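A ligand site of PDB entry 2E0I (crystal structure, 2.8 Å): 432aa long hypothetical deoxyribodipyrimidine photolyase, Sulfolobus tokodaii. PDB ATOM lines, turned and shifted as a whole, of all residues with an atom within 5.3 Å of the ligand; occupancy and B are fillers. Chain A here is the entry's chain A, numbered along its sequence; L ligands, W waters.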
ATOM      1  N   PHE A   7       2.185  -2.514  19.528  1.00  0.00           N
ATOM      2  CA  PHE A   7       1.853  -1.998  20.856  1.00  0.00           C
ATOM      3  C   PHE A   7       0.860  -0.866  20.649  1.00  0.00           C
ATOM      4  O   PHE A   7       0.864  -0.199  19.613  1.00  0.00           O
ATOM      5  CB  PHE A   7       3.077  -1.420  21.555  1.00  0.00           C
ATOM      6  CG  PHE A   7       4.081  -2.441  21.952  1.00  0.00           C
ATOM      7  CD1 PHE A   7       4.019  -3.033  23.209  1.00  0.00           C
ATOM      8  CD2 PHE A   7       5.093  -2.826  21.075  1.00  0.00           C
ATOM      9  CE1 PHE A   7       4.957  -3.979  23.593  1.00  0.00           C
ATOM     10  CE2 PHE A   7       6.036  -3.780  21.455  1.00  0.00           C
ATOM     11  CZ  PHE A   7       5.965  -4.356  22.722  1.00  0.00           C
ATOM     12  N   ARG A   8       0.018  -0.622  21.636  1.00  0.00           N
ATOM     13  CA  ARG A   8      -0.925   0.473  21.536  1.00  0.00           C
ATOM     14  C   ARG A   8      -1.191   1.077  22.894  1.00  0.00           C
ATOM     15  O   ARG A   8      -0.949   2.265  23.103  1.00  0.00           O
ATOM     16  CB  ARG A   8      -2.243  -0.014  20.937  1.00  0.00           C
ATOM     17  CG  ARG A   8      -2.120  -0.587  19.539  1.00  0.00           C
ATOM     18  CD  ARG A   8      -2.996  -1.797  19.457  1.00  0.00           C
ATOM     19  NE  ARG A   8      -3.726  -1.824  18.205  1.00  0.00           N
ATOM     20  CZ  ARG A   8      -4.862  -2.487  18.029  1.00  0.00           C
ATOM     21  NH1 ARG A   8      -5.390  -3.186  19.046  1.00  0.00           N
ATOM     22  NH2 ARG A   8      -5.475  -2.452  16.853  1.00  0.00           N
ATOM     23  N   ARG A   9      -1.637   0.239  23.810  1.00  0.00           N
ATOM     24  CA  ARG A   9      -2.031   0.633  25.161  1.00  0.00           C
ATOM     25  C   ARG A   9      -1.501  -0.380  26.163  1.00  0.00           C
ATOM     26  O   ARG A   9      -1.917  -0.390  27.328  1.00  0.00           O
ATOM     27  CB  ARG A   9      -3.554   0.573  25.198  1.00  0.00           C
ATOM     28  CG  ARG A   9      -4.270   1.708  25.769  1.00  0.00           C
ATOM     29  CD  ARG A   9      -5.766   1.442  25.570  1.00  0.00           C
ATOM     30  NE  ARG A   9      -6.206   1.093  26.877  1.00  0.00           N
ATOM     31  CZ  ARG A   9      -7.049   0.166  27.303  1.00  0.00           C
ATOM     32  NH1 ARG A   9      -7.162   0.158  28.608  1.00  0.00           N
ATOM     33  NH2 ARG A   9      -7.736  -0.692  26.555  1.00  0.00           N
ATOM     34  N   PHE A  33       5.201   0.385  17.054  1.00  0.00           N
ATOM     35  CA  PHE A  33       4.271   1.357  17.627  1.00  0.00           C
ATOM     36  C   PHE A  33       3.967   2.347  16.502  1.00  0.00           C
ATOM     37  O   PHE A  33       4.881   2.873  15.872  1.00  0.00           O
ATOM     38  CB  PHE A  33       4.826   2.124  18.821  1.00  0.00           C
ATOM     39  CG  PHE A  33       3.875   3.169  19.323  1.00  0.00           C
ATOM     40  CD1 PHE A  33       3.985   4.495  18.887  1.00  0.00           C
ATOM     41  CD2 PHE A  33       2.824   2.824  20.165  1.00  0.00           C
ATOM     42  CE1 PHE A  33       3.051   5.482  19.289  1.00  0.00           C
ATOM     43  CE2 PHE A  33       1.876   3.798  20.574  1.00  0.00           C
ATOM     44  CZ  PHE A  33       1.998   5.123  20.130  1.00  0.00           C
ATOM     45  N   ILE A  34       2.685   2.586  16.253  1.00  0.00           N
ATOM     46  CA  ILE A  34       2.276   3.477  15.200  1.00  0.00           C
ATOM     47  C   ILE A  34       1.705   4.773  15.745  1.00  0.00           C
ATOM     48  O   ILE A  34       0.694   4.756  16.454  1.00  0.00           O
ATOM     49  CB  ILE A  34       1.214   2.813  14.314  1.00  0.00           C
ATOM     50  CG1 ILE A  34       1.792   1.546  13.669  1.00  0.00           C
ATOM     51  CG2 ILE A  34       0.714   3.797  13.259  1.00  0.00           C
ATOM     52  CD1 ILE A  34       0.780   0.744  12.897  1.00  0.00           C
ATOM     53  N   ALA A  35       2.360   5.884  15.417  1.00  0.00           N
ATOM     54  CA  ALA A  35       1.911   7.208  15.850  1.00  0.00           C
ATOM     55  C   ALA A  35       0.800   7.598  14.872  1.00  0.00           C
ATOM     56  O   ALA A  35       1.059   7.868  13.697  1.00  0.00           O
ATOM     57  CB  ALA A  35       3.056   8.206  15.768  1.00  0.00           C
ATOM     58  N   ASP A  36      -0.444   7.589  15.366  1.00  0.00           N
ATOM     59  CA  ASP A  36      -1.611   7.874  14.536  1.00  0.00           C
ATOM     60  C   ASP A  36      -2.064   9.334  14.633  1.00  0.00           C
ATOM     61  O   ASP A  36      -2.444   9.820  15.713  1.00  0.00           O
ATOM     62  CB  ASP A  36      -2.749   6.926  14.938  1.00  0.00           C
ATOM     63  CG  ASP A  36      -3.925   6.973  13.969  1.00  0.00           C
ATOM     64  OD1 ASP A  36      -4.548   5.899  13.737  1.00  0.00           O
ATOM     65  OD2 ASP A  36      -4.246   8.065  13.456  1.00  0.00           O
ATOM     66  N   ARG A  38      -4.729  10.698  13.898  1.00  0.00           N
ATOM     67  CA  ARG A  38      -6.123  10.843  14.344  1.00  0.00           C
ATOM     68  C   ARG A  38      -6.178  10.953  15.855  1.00  0.00           C
ATOM     69  O   ARG A  38      -7.161  11.418  16.409  1.00  0.00           O
ATOM     70  CB  ARG A  38      -6.973   9.653  13.906  1.00  0.00           C
ATOM     71  CG  ARG A  38      -7.106   9.534  12.394  1.00  0.00           C
ATOM     72  CD  ARG A  38      -7.769   8.266  11.967  1.00  0.00           C
ATOM     73  NE  ARG A  38      -6.956   7.106  12.290  1.00  0.00           N
ATOM     74  CZ  ARG A  38      -7.273   5.867  11.963  1.00  0.00           C
ATOM     75  NH1 ARG A  38      -8.387   5.614  11.306  1.00  0.00           N
ATOM     76  NH2 ARG A  38      -6.485   4.858  12.321  1.00  0.00           N
ATOM     77  N   GLN A  39      -5.096  10.516  16.505  1.00  0.00           N
ATOM     78  CA  GLN A  39      -4.996  10.538  17.948  1.00  0.00           C
ATOM     79  C   GLN A  39      -4.031  11.622  18.431  1.00  0.00           C
ATOM     80  O   GLN A  39      -4.244  12.216  19.484  1.00  0.00           O
ATOM     81  CB  GLN A  39      -4.533   9.168  18.466  1.00  0.00           C
ATOM     82  CG  GLN A  39      -5.532   8.043  18.177  1.00  0.00           C
ATOM     83  CD  GLN A  39      -5.021   6.668  18.582  1.00  0.00           C
ATOM     84  OE1 GLN A  39      -4.104   6.119  17.948  1.00  0.00           O
ATOM     85  NE2 GLN A  39      -5.599   6.103  19.636  1.00  0.00           N
ATOM     86  N   LEU A  40      -2.972  11.872  17.679  1.00  0.00           N
ATOM     87  CA  LEU A  40      -1.987  12.858  18.103  1.00  0.00           C
ATOM     88  C   LEU A  40      -2.102  14.276  17.537  1.00  0.00           C
ATOM     89  O   LEU A  40      -1.559  15.224  18.132  1.00  0.00           O
ATOM     90  CB  LEU A  40      -0.595  12.327  17.813  1.00  0.00           C
ATOM     91  CG  LEU A  40      -0.235  11.038  18.561  1.00  0.00           C
ATOM     92  CD1 LEU A  40       1.082  10.489  18.020  1.00  0.00           C
ATOM     93  CD2 LEU A  40      -0.122  11.303  20.078  1.00  0.00           C
ATOM     94  N   ASN A  43      -6.982  16.264  17.874  1.00  0.00           N
ATOM     95  CA  ASN A  43      -7.817  15.328  18.569  1.00  0.00           C
ATOM     96  C   ASN A  43      -8.487  16.201  19.624  1.00  0.00           C
ATOM     97  O   ASN A  43      -7.843  16.706  20.539  1.00  0.00           O
ATOM     98  CB  ASN A  43      -6.951  14.254  19.222  1.00  0.00           C
ATOM     99  CG  ASN A  43      -7.741  13.338  20.115  1.00  0.00           C
ATOM    100  OD1 ASN A  43      -8.901  13.606  20.411  1.00  0.00           O
ATOM    101  ND2 ASN A  43      -7.124  12.254  20.548  1.00  0.00           N
ATOM    102  N   PRO A  44      -9.791  16.426  19.476  1.00  0.00           N
ATOM    103  CA  PRO A  44     -10.464  17.255  20.473  1.00  0.00           C
ATOM    104  C   PRO A  44     -10.395  16.638  21.894  1.00  0.00           C
ATOM    105  O   PRO A  44     -10.474  17.339  22.891  1.00  0.00           O
ATOM    106  CB  PRO A  44     -11.898  17.343  19.956  1.00  0.00           C
ATOM    107  CG  PRO A  44     -11.755  17.068  18.473  1.00  0.00           C
ATOM    108  CD  PRO A  44     -10.728  15.988  18.426  1.00  0.00           C
ATOM    109  N   TYR A  45     -10.237  15.321  21.955  1.00  0.00           N
ATOM    110  CA  TYR A  45     -10.215  14.616  23.217  1.00  0.00           C
ATOM    111  C   TYR A  45      -8.803  14.290  23.706  1.00  0.00           C
ATOM    112  O   TYR A  45      -8.612  13.437  24.574  1.00  0.00           O
ATOM    113  CB  TYR A  45     -11.028  13.331  23.086  1.00  0.00           C
ATOM    114  CG  TYR A  45     -12.511  13.580  23.039  1.00  0.00           C
ATOM    115  CD1 TYR A  45     -13.293  13.423  24.182  1.00  0.00           C
ATOM    116  CD2 TYR A  45     -13.138  13.982  21.867  1.00  0.00           C
ATOM    117  CE1 TYR A  45     -14.665  13.668  24.165  1.00  0.00           C
ATOM    118  CE2 TYR A  45     -14.509  14.236  21.838  1.00  0.00           C
ATOM    119  CZ  TYR A  45     -15.263  14.067  22.984  1.00  0.00           C
ATOM    120  OH  TYR A  45     -16.621  14.291  22.952  1.00  0.00           O
ATOM    121  N   LYS A  46      -7.823  14.978  23.158  1.00  0.00           N
ATOM    122  CA  LYS A  46      -6.447  14.716  23.535  1.00  0.00           C
ATOM    123  C   LYS A  46      -5.985  15.464  24.770  1.00  0.00           C
ATOM    124  O   LYS A  46      -6.349  16.615  24.994  1.00  0.00           O
ATOM    125  CB  LYS A  46      -5.512  15.020  22.356  1.00  0.00           C
ATOM    126  CG  LYS A  46      -4.039  14.997  22.706  1.00  0.00           C
ATOM    127  CD  LYS A  46      -3.207  15.528  21.557  1.00  0.00           C
ATOM    128  CE  LYS A  46      -1.803  15.907  22.010  1.00  0.00           C
ATOM    129  NZ  LYS A  46      -0.950  16.412  20.879  1.00  0.00           N
ATOM    130  N   SER A  47      -5.201  14.776  25.582  1.00  0.00           N
ATOM    131  CA  SER A  47      -4.647  15.312  26.797  1.00  0.00           C
ATOM    132  C   SER A  47      -3.129  15.414  26.608  1.00  0.00           C
ATOM    133  O   SER A  47      -2.491  14.432  26.225  1.00  0.00           O
ATOM    134  CB  SER A  47      -4.986  14.387  27.970  1.00  0.00           C
ATOM    135  OG  SER A  47      -4.276  14.754  29.138  1.00  0.00           O
ATOM    136  N   ALA A  50      -1.495  13.115  29.293  1.00  0.00           N
ATOM    137  CA  ALA A  50      -1.591  11.703  28.946  1.00  0.00           C
ATOM    138  C   ALA A  50      -0.572  11.327  27.878  1.00  0.00           C
ATOM    139  O   ALA A  50       0.072  10.276  27.956  1.00  0.00           O
ATOM    140  CB  ALA A  50      -2.981  11.398  28.435  1.00  0.00           C
ATOM    141  N   VAL A  51      -0.423  12.192  26.885  1.00  0.00           N
ATOM    142  CA  VAL A  51       0.509  11.951  25.793  1.00  0.00           C
ATOM    143  C   VAL A  51       1.950  11.871  26.283  1.00  0.00           C
ATOM    144  O   VAL A  51       2.711  10.989  25.865  1.00  0.00           O
ATOM    145  CB  VAL A  51       0.349  13.039  24.720  1.00  0.00           C
ATOM    146  CG1 VAL A  51       1.397  12.873  23.644  1.00  0.00           C
ATOM    147  CG2 VAL A  51      -1.018  12.926  24.101  1.00  0.00           C
ATOM    148  N   MET A  54       2.522   8.639  27.955  1.00  0.00           N
ATOM    149  CA  MET A  54       2.626   7.568  26.970  1.00  0.00           C
ATOM    150  C   MET A  54       4.011   7.586  26.309  1.00  0.00           C
ATOM    151  O   MET A  54       4.686   6.553  26.204  1.00  0.00           O
ATOM    152  CB  MET A  54       1.523   7.739  25.944  1.00  0.00           C
ATOM    153  CG  MET A  54       1.486   6.679  24.889  1.00  0.00           C
ATOM    154  SD  MET A  54       0.220   7.102  23.692  1.00  0.00           S
ATOM    155  CE  MET A  54       1.149   8.187  22.614  1.00  0.00           C
ATOM    156  N   ASP A  98      -9.088  -3.987  21.580  1.00  0.00           N
ATOM    157  CA  ASP A  98      -9.545  -2.977  22.527  1.00  0.00           C
ATOM    158  C   ASP A  98     -11.064  -2.967  22.398  1.00  0.00           C
ATOM    159  O   ASP A  98     -11.624  -3.740  21.621  1.00  0.00           O
ATOM    160  CB  ASP A  98      -8.955  -1.588  22.225  1.00  0.00           C
ATOM    161  CG  ASP A  98      -8.848  -0.705  23.472  1.00  0.00           C
ATOM    162  OD1 ASP A  98      -9.695  -0.819  24.383  1.00  0.00           O
ATOM    163  OD2 ASP A  98      -7.915   0.118  23.539  1.00  0.00           O
ATOM    164  N   THR A 100     -13.296   0.112  22.094  1.00  0.00           N
ATOM    165  CA  THR A 100     -13.994   1.351  21.738  1.00  0.00           C
ATOM    166  C   THR A 100     -14.270   1.373  20.246  1.00  0.00           C
ATOM    167  O   THR A 100     -13.556   0.751  19.446  1.00  0.00           O
ATOM    168  CB  THR A 100     -13.182   2.630  22.045  1.00  0.00           C
ATOM    169  OG1 THR A 100     -11.919   2.573  21.359  1.00  0.00           O
ATOM    170  CG2 THR A 100     -12.952   2.788  23.529  1.00  0.00           C
ATOM    171  N   PHE A 102     -13.683   3.416  17.890  1.00  0.00           N
ATOM    172  CA  PHE A 102     -12.490   3.755  17.131  1.00  0.00           C
ATOM    173  C   PHE A 102     -11.563   2.566  17.010  1.00  0.00           C
ATOM    174  O   PHE A 102     -11.027   2.280  15.940  1.00  0.00           O
ATOM    175  CB  PHE A 102     -11.746   4.928  17.782  1.00  0.00           C
ATOM    176  CG  PHE A 102     -10.388   5.194  17.188  1.00  0.00           C
ATOM    177  CD1 PHE A 102      -9.263   4.556  17.694  1.00  0.00           C
ATOM    178  CD2 PHE A 102     -10.254   6.055  16.105  1.00  0.00           C
ATOM    179  CE1 PHE A 102      -7.999   4.776  17.123  1.00  0.00           C
ATOM    180  CE2 PHE A 102      -9.010   6.293  15.528  1.00  0.00           C
ATOM    181  CZ  PHE A 102      -7.875   5.645  16.036  1.00  0.00           C
ATOM    182  N   SER A 103     -11.371   1.865  18.121  1.00  0.00           N
ATOM    183  CA  SER A 103     -10.485   0.723  18.116  1.00  0.00           C
ATOM    184  C   SER A 103     -11.035  -0.437  17.322  1.00  0.00           C
ATOM    185  O   SER A 103     -10.305  -1.143  16.645  1.00  0.00           O
ATOM    186  CB  SER A 103     -10.225   0.265  19.538  1.00  0.00           C
ATOM    187  OG  SER A 103      -9.453  -0.922  19.494  1.00  0.00           O
ATOM    188  N   ARG A 106     -10.873   0.367  13.548  1.00  0.00           N
ATOM    189  CA  ARG A 106      -9.474   0.424  13.148  1.00  0.00           C
ATOM    190  C   ARG A 106      -8.935  -0.972  12.912  1.00  0.00           C
ATOM    191  O   ARG A 106      -8.153  -1.206  11.997  1.00  0.00           O
ATOM    192  CB  ARG A 106      -8.677   1.110  14.223  1.00  0.00           C
ATOM    193  CG  ARG A 106      -7.202   0.786  14.313  1.00  0.00           C
ATOM    194  CD  ARG A 106      -6.783   1.819  15.218  1.00  0.00           C
ATOM    195  NE  ARG A 106      -5.945   1.603  16.369  1.00  0.00           N
ATOM    196  CZ  ARG A 106      -6.185   1.085  17.571  1.00  0.00           C
ATOM    197  NH1 ARG A 106      -5.164   1.137  18.385  1.00  0.00           N
ATOM    198  NH2 ARG A 106      -7.301   0.505  17.988  1.00  0.00           N
ATOM    199  N   LYS A 221      -4.081   2.178  32.548  1.00  0.00           N
ATOM    200  CA  LYS A 221      -4.628   2.628  31.276  1.00  0.00           C
ATOM    201  C   LYS A 221      -3.619   2.452  30.139  1.00  0.00           C
ATOM    202  O   LYS A 221      -3.998   2.009  29.052  1.00  0.00           O
ATOM    203  CB  LYS A 221      -5.056   4.097  31.406  1.00  0.00           C
ATOM    204  CG  LYS A 221      -4.770   4.990  30.190  1.00  0.00           C
ATOM    205  CD  LYS A 221      -5.673   4.699  29.029  1.00  0.00           C
ATOM    206  CE  LYS A 221      -5.248   5.500  27.819  1.00  0.00           C
ATOM    207  NZ  LYS A 221      -6.323   5.496  26.777  1.00  0.00           N
ATOM    208  N   PHE A 222      -2.353   2.776  30.381  1.00  0.00           N
ATOM    209  CA  PHE A 222      -1.342   2.628  29.325  1.00  0.00           C
ATOM    210  C   PHE A 222      -0.615   1.304  29.365  1.00  0.00           C
ATOM    211  O   PHE A 222       0.272   1.047  28.544  1.00  0.00           O
ATOM    212  CB  PHE A 222      -0.380   3.801  29.360  1.00  0.00           C
ATOM    213  CG  PHE A 222      -0.909   5.029  28.688  1.00  0.00           C
ATOM    214  CD1 PHE A 222      -1.071   5.053  27.300  1.00  0.00           C
ATOM    215  CD2 PHE A 222      -1.302   6.133  29.429  1.00  0.00           C
ATOM    216  CE1 PHE A 222      -1.604   6.165  26.659  1.00  0.00           C
ATOM    217  CE2 PHE A 222      -1.834   7.250  28.801  1.00  0.00           C
ATOM    218  CZ  PHE A 222      -1.986   7.260  27.403  1.00  0.00           C
ATOM    219  N   PHE A 261     -21.084   6.717  23.891  1.00  0.00           N
ATOM    220  CA  PHE A 261     -20.196   7.745  23.374  1.00  0.00           C
ATOM    221  C   PHE A 261     -20.972   8.716  22.509  1.00  0.00           C
ATOM    222  O   PHE A 261     -21.003   8.586  21.298  1.00  0.00           O
ATOM    223  CB  PHE A 261     -19.077   7.096  22.571  1.00  0.00           C
ATOM    224  CG  PHE A 261     -18.147   6.277  23.413  1.00  0.00           C
ATOM    225  CD1 PHE A 261     -17.453   6.856  24.469  1.00  0.00           C
ATOM    226  CD2 PHE A 261     -17.976   4.920  23.156  1.00  0.00           C
ATOM    227  CE1 PHE A 261     -16.602   6.104  25.257  1.00  0.00           C
ATOM    228  CE2 PHE A 261     -17.121   4.160  23.939  1.00  0.00           C
ATOM    229  CZ  PHE A 261     -16.436   4.754  25.004  1.00  0.00           C
ATOM    230  N   GLU A 331     -17.117  15.711  30.244  1.00  0.00           N
ATOM    231  CA  GLU A 331     -16.436  14.506  29.787  1.00  0.00           C
ATOM    232  C   GLU A 331     -15.277  14.891  28.885  1.00  0.00           C
ATOM    233  O   GLU A 331     -14.150  14.429  29.081  1.00  0.00           O
ATOM    234  CB  GLU A 331     -17.391  13.627  28.982  1.00  0.00           C
ATOM    235  CG  GLU A 331     -16.723  12.407  28.393  1.00  0.00           C
ATOM    236  CD  GLU A 331     -17.537  11.734  27.282  1.00  0.00           C
ATOM    237  OE1 GLU A 331     -17.134  10.624  26.849  1.00  0.00           O
ATOM    238  OE2 GLU A 331     -18.550  12.323  26.836  1.00  0.00           O
ATOM    239  N   TYR A 341      -6.626   9.469  31.094  1.00  0.00           N
ATOM    240  CA  TYR A 341      -7.837   9.393  30.279  1.00  0.00           C
ATOM    241  C   TYR A 341      -8.156   8.052  29.632  1.00  0.00           C
ATOM    242  O   TYR A 341      -7.367   7.505  28.853  1.00  0.00           O
ATOM    243  CB  TYR A 341      -7.814  10.464  29.179  1.00  0.00           C
ATOM    244  CG  TYR A 341      -9.024  10.374  28.284  1.00  0.00           C
ATOM    245  CD1 TYR A 341      -8.895  10.047  26.929  1.00  0.00           C
ATOM    246  CD2 TYR A 341     -10.308  10.578  28.786  1.00  0.00           C
ATOM    247  CE1 TYR A 341     -10.013   9.923  26.111  1.00  0.00           C
ATOM    248  CE2 TYR A 341     -11.426  10.460  27.981  1.00  0.00           C
ATOM    249  CZ  TYR A 341     -11.279  10.128  26.649  1.00  0.00           C
ATOM    250  OH  TYR A 341     -12.383  10.015  25.848  1.00  0.00           O
ATOM    251  N   PRO A 343     -11.434   6.591  27.557  1.00  0.00           N
ATOM    252  CA  PRO A 343     -12.763   6.863  26.983  1.00  0.00           C
ATOM    253  C   PRO A 343     -13.940   6.230  27.713  1.00  0.00           C
ATOM    254  O   PRO A 343     -14.854   6.933  28.135  1.00  0.00           O
ATOM    255  CB  PRO A 343     -12.612   6.375  25.544  1.00  0.00           C
ATOM    256  CG  PRO A 343     -11.180   6.642  25.248  1.00  0.00           C
ATOM    257  CD  PRO A 343     -10.490   6.174  26.499  1.00  0.00           C
HETATM  258  P1  LIG L   1      -8.143   7.696  21.841  1.00  0.00           P
HETATM  259  O1  LIG L   1      -8.898   8.044  23.061  1.00  0.00           O
HETATM  260  O2  LIG L   1      -6.883   8.350  21.406  1.00  0.00           O
HETATM  261  O3  LIG L   1      -9.127   8.425  20.795  1.00  0.00           O
HETATM  262  C1  LIG L   1      -9.021   8.155  19.392  1.00  0.00           C
HETATM  263  C2  LIG L   1     -10.142   8.846  18.604  1.00  0.00           C
HETATM  264  O4  LIG L   1     -11.347   8.792  19.389  1.00  0.00           O
HETATM  265  C3  LIG L   1      -9.840  10.326  18.383  1.00  0.00           C
HETATM  266  O5  LIG L   1     -10.576  10.805  17.256  1.00  0.00           O
HETATM  267  C4  LIG L   1     -10.400  10.928  19.669  1.00  0.00           C
HETATM  268  O6  LIG L   1     -10.718  12.309  19.461  1.00  0.00           O
HETATM  269  C5  LIG L   1     -11.707  10.137  19.773  1.00  0.00           C
HETATM  270  N1  LIG L   1     -12.278  10.181  21.138  1.00  0.00           N
HETATM  271  C6  LIG L   1     -11.632   9.888  22.266  1.00  0.00           C
HETATM  272  N2  LIG L   1     -12.470   9.984  23.298  1.00  0.00           N
HETATM  273  C7  LIG L   1     -13.655  10.341  22.835  1.00  0.00           C
HETATM  274  C8  LIG L   1     -14.898  10.576  23.412  1.00  0.00           C
HETATM  275  N3  LIG L   1     -15.056  10.495  24.725  1.00  0.00           N
HETATM  276  N4  LIG L   1     -15.927  10.916  22.629  1.00  0.00           N
HETATM  277  C9  LIG L   1     -15.780  11.041  21.321  1.00  0.00           C
HETATM  278  N5  LIG L   1     -14.616  10.833  20.731  1.00  0.00           N
HETATM  279  C10 LIG L   1     -13.544  10.477  21.455  1.00  0.00           C
HETATM  280  N6  LIG L   1      -2.131   4.517  20.551  1.00  0.00           N
HETATM  281  C11 LIG L   1      -1.446   4.285  19.355  1.00  0.00           C
HETATM  282  O7  LIG L   1      -1.323   3.136  18.920  1.00  0.00           O
HETATM  283  N7  LIG L   1      -0.943   5.365  18.618  1.00  0.00           N
HETATM  284  C12 LIG L   1      -1.130   6.679  19.069  1.00  0.00           C
HETATM  285  O8  LIG L   1      -0.677   7.622  18.432  1.00  0.00           O
HETATM  286  C13 LIG L   1      -1.827   6.907  20.261  1.00  0.00           C
HETATM  287  N8  LIG L   1      -2.074   8.218  20.680  1.00  0.00           N
HETATM  288  C14 LIG L   1      -2.800   8.451  21.856  1.00  0.00           C
HETATM  289  C15 LIG L   1      -3.125   9.763  22.220  1.00  0.00           C
HETATM  290  C16 LIG L   1      -3.922  10.004  23.337  1.00  0.00           C
HETATM  291  C17 LIG L   1      -4.263  11.447  23.713  1.00  0.00           C
HETATM  292  C18 LIG L   1      -4.394   8.933  24.090  1.00  0.00           C
HETATM  293  C19 LIG L   1      -5.265   9.160  25.323  1.00  0.00           C
HETATM  294  C20 LIG L   1      -4.057   7.625  23.731  1.00  0.00           C
HETATM  295  C21 LIG L   1      -3.267   7.378  22.618  1.00  0.00           C
HETATM  296  N9  LIG L   1      -2.971   6.073  22.214  1.00  0.00           N
HETATM  297  C22 LIG L   1      -2.324   5.833  20.994  1.00  0.00           C
HETATM  298  C23 LIG L   1      -3.431   4.909  23.016  1.00  0.00           C
HETATM  299  C24 LIG L   1      -4.888   4.529  22.741  1.00  0.00           C
HETATM  300  O9  LIG L   1      -5.607   4.499  23.976  1.00  0.00           O
HETATM  301  C25 LIG L   1      -4.956   3.157  22.053  1.00  0.00           C
HETATM  302  O10 LIG L   1      -4.329   3.240  20.772  1.00  0.00           O
HETATM  303  C26 LIG L   1      -6.412   2.711  21.879  1.00  0.00           C
HETATM  304  O11 LIG L   1      -6.434   1.354  21.437  1.00  0.00           O
HETATM  305  C27 LIG L   1      -7.134   3.601  20.858  1.00  0.00           C
HETATM  306  O12 LIG L   1      -8.524   3.756  21.190  1.00  0.00           O
HETATM  307  P2  LIG L   1      -8.996   5.009  22.080  1.00  0.00           P
HETATM  308  O13 LIG L   1     -10.471   5.027  22.045  1.00  0.00           O
HETATM  309  O14 LIG L   1      -8.327   4.967  23.402  1.00  0.00           O
HETATM  310  O15 LIG L   1      -8.447   6.244  21.213  1.00  0.00           O
HETATM  311  O   HOH W   1      -9.332   2.826  24.992  1.00  0.00           O
HETATM  312  O   HOH W   2      -9.198  13.140  15.892  1.00  0.00           O
HETATM  313  O   HOH W   3      -6.415  12.313  25.980  1.00  0.00           O
HETATM  314  O   HOH W   4      -7.887  11.102  23.002  1.00  0.00           O
HETATM  315  O   HOH W   5       0.700   1.587  18.006  1.00  0.00           O
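Water W5 lies within hydrogen-bond range of O of Phe 7 (2.4 Å), O7 of the ligand (2.7 Å) and N of Ile 34 (2.8 Å).
Water W1 lies within hydrogen-bond range of O14 of the ligand (2.8 Å) and OD2 of Asp 98 (3.4 Å).
Water W2 bridges O of Arg 38 (2.7 Å) and O5 of the ligand (3.0 Å).
Water W4 lies within hydrogen-bond range of ND2 of Asn 43, O of Tyr 45 and O1 of the ligand.
The guanidinium group of Arg 38 is in salt-bridge range of the side-chain carboxylate of Asp 36, at 2.6 Å.
The side-chain amide nitrogen (ND2) of Asn 43 is in hydrogen-bond range of the backbone carbonyl oxygen (O) of Gln 39 (3.1 Å).
OG1 of Thr 100 sits at hydrogen-bond distance from N of Ser 103.
The backbone NH of Ala 50 is in hydrogen-bond range of the side-chain hydroxyl of Ser 47 (3.2 Å).
The side-chain amide oxygen (OD1) of Asn 43 is in hydrogen-bond range of the backbone NH (N) of Tyr 45 (2.7 Å).
The side-chain amino group (NZ) of Lys 46 is in hydrogen-bond range of the backbone carbonyl oxygen (O) of Leu 40, at 3.1 Å.
The backbone carbonyl oxygen of Lys 221 lies within hydrogen-bond range of the guanidinium group of Arg 9 (3.2 Å).
The side-chain amino group of Lys 221 is in hydrogen-bond range of the backbone carbonyl oxygen of Tyr 341, 3.1 Å away.
The side-chain sulfur (SD) of Met 54 lies close to a nitrogen (N9) of the ligand (3.7 Å).
Merely in contact with the ligand: Phe 33, Leu 40, Arg 9, Pro 343, Arg 38, Val 51, Arg 8, Phe 102, Ala 35, Lys 46, Pro 44 and Ser 47.
Hydrophobic or aromatic side chains that line the ligand: Phe 33, Leu 40, Pro 44, Tyr 45, Val 51, Met 54, Phe 102, Tyr 341 and Pro 343.
24 residues have an atom within 4 Å of the ligand: Arg 8, Arg 9, Phe 33, Ile 34, Ala 35, Asp 36, Arg 38, Gln 39, Leu 40, Asn 43, Pro 44, Tyr 45, Lys 46, Ser 47, Val 51, Met 54, Asp 98, Thr 100, Phe 102, Arg 106, Lys 221, Glu 331, Tyr 341 and Pro 343.
A nitrogen (N3) of the ligand lies within hydrogen-bond range of the side-chain carboxylate of Glu 331, at 3.0 Å.
OD1 of Asn 43 lies within hydrogen-bond range of O6 of the ligand (2.4 Å).
The guanidinium group (NH1) of Arg 106 is in hydrogen-bond range of an oxygen (O10) of the ligand.
The side-chain amino group of Lys 221 is in salt-bridge range of an oxygen (O14) of the ligand, at 3.96 Å.
The side-chain hydroxyl (OH) of Tyr 45 sits close to a nitrogen (N4) of the ligand.
O2 of the ligand sits at hydrogen-bond distance from NE2 of Gln 39, at 3.1 Å.
The backbone carbonyl oxygen (O) of Ile 34 sits at hydrogen-bond distance from a nitrogen (N7) of the ligand (2.8 Å).
OH of Tyr 341 is in hydrogen-bond range of N2 of the ligand.
The side-chain carboxylate of Asp 98 lies within hydrogen-bond range of an oxygen (O11) of the ligand (2.9 Å).
An oxygen (O13) of the ligand lies within hydrogen-bond range of the side-chain hydroxyl (OG1) of Thr 100, at 2.9 Å.
The backbone NH of Asp 36 is in hydrogen-bond range of an oxygen (O8) of the ligand.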
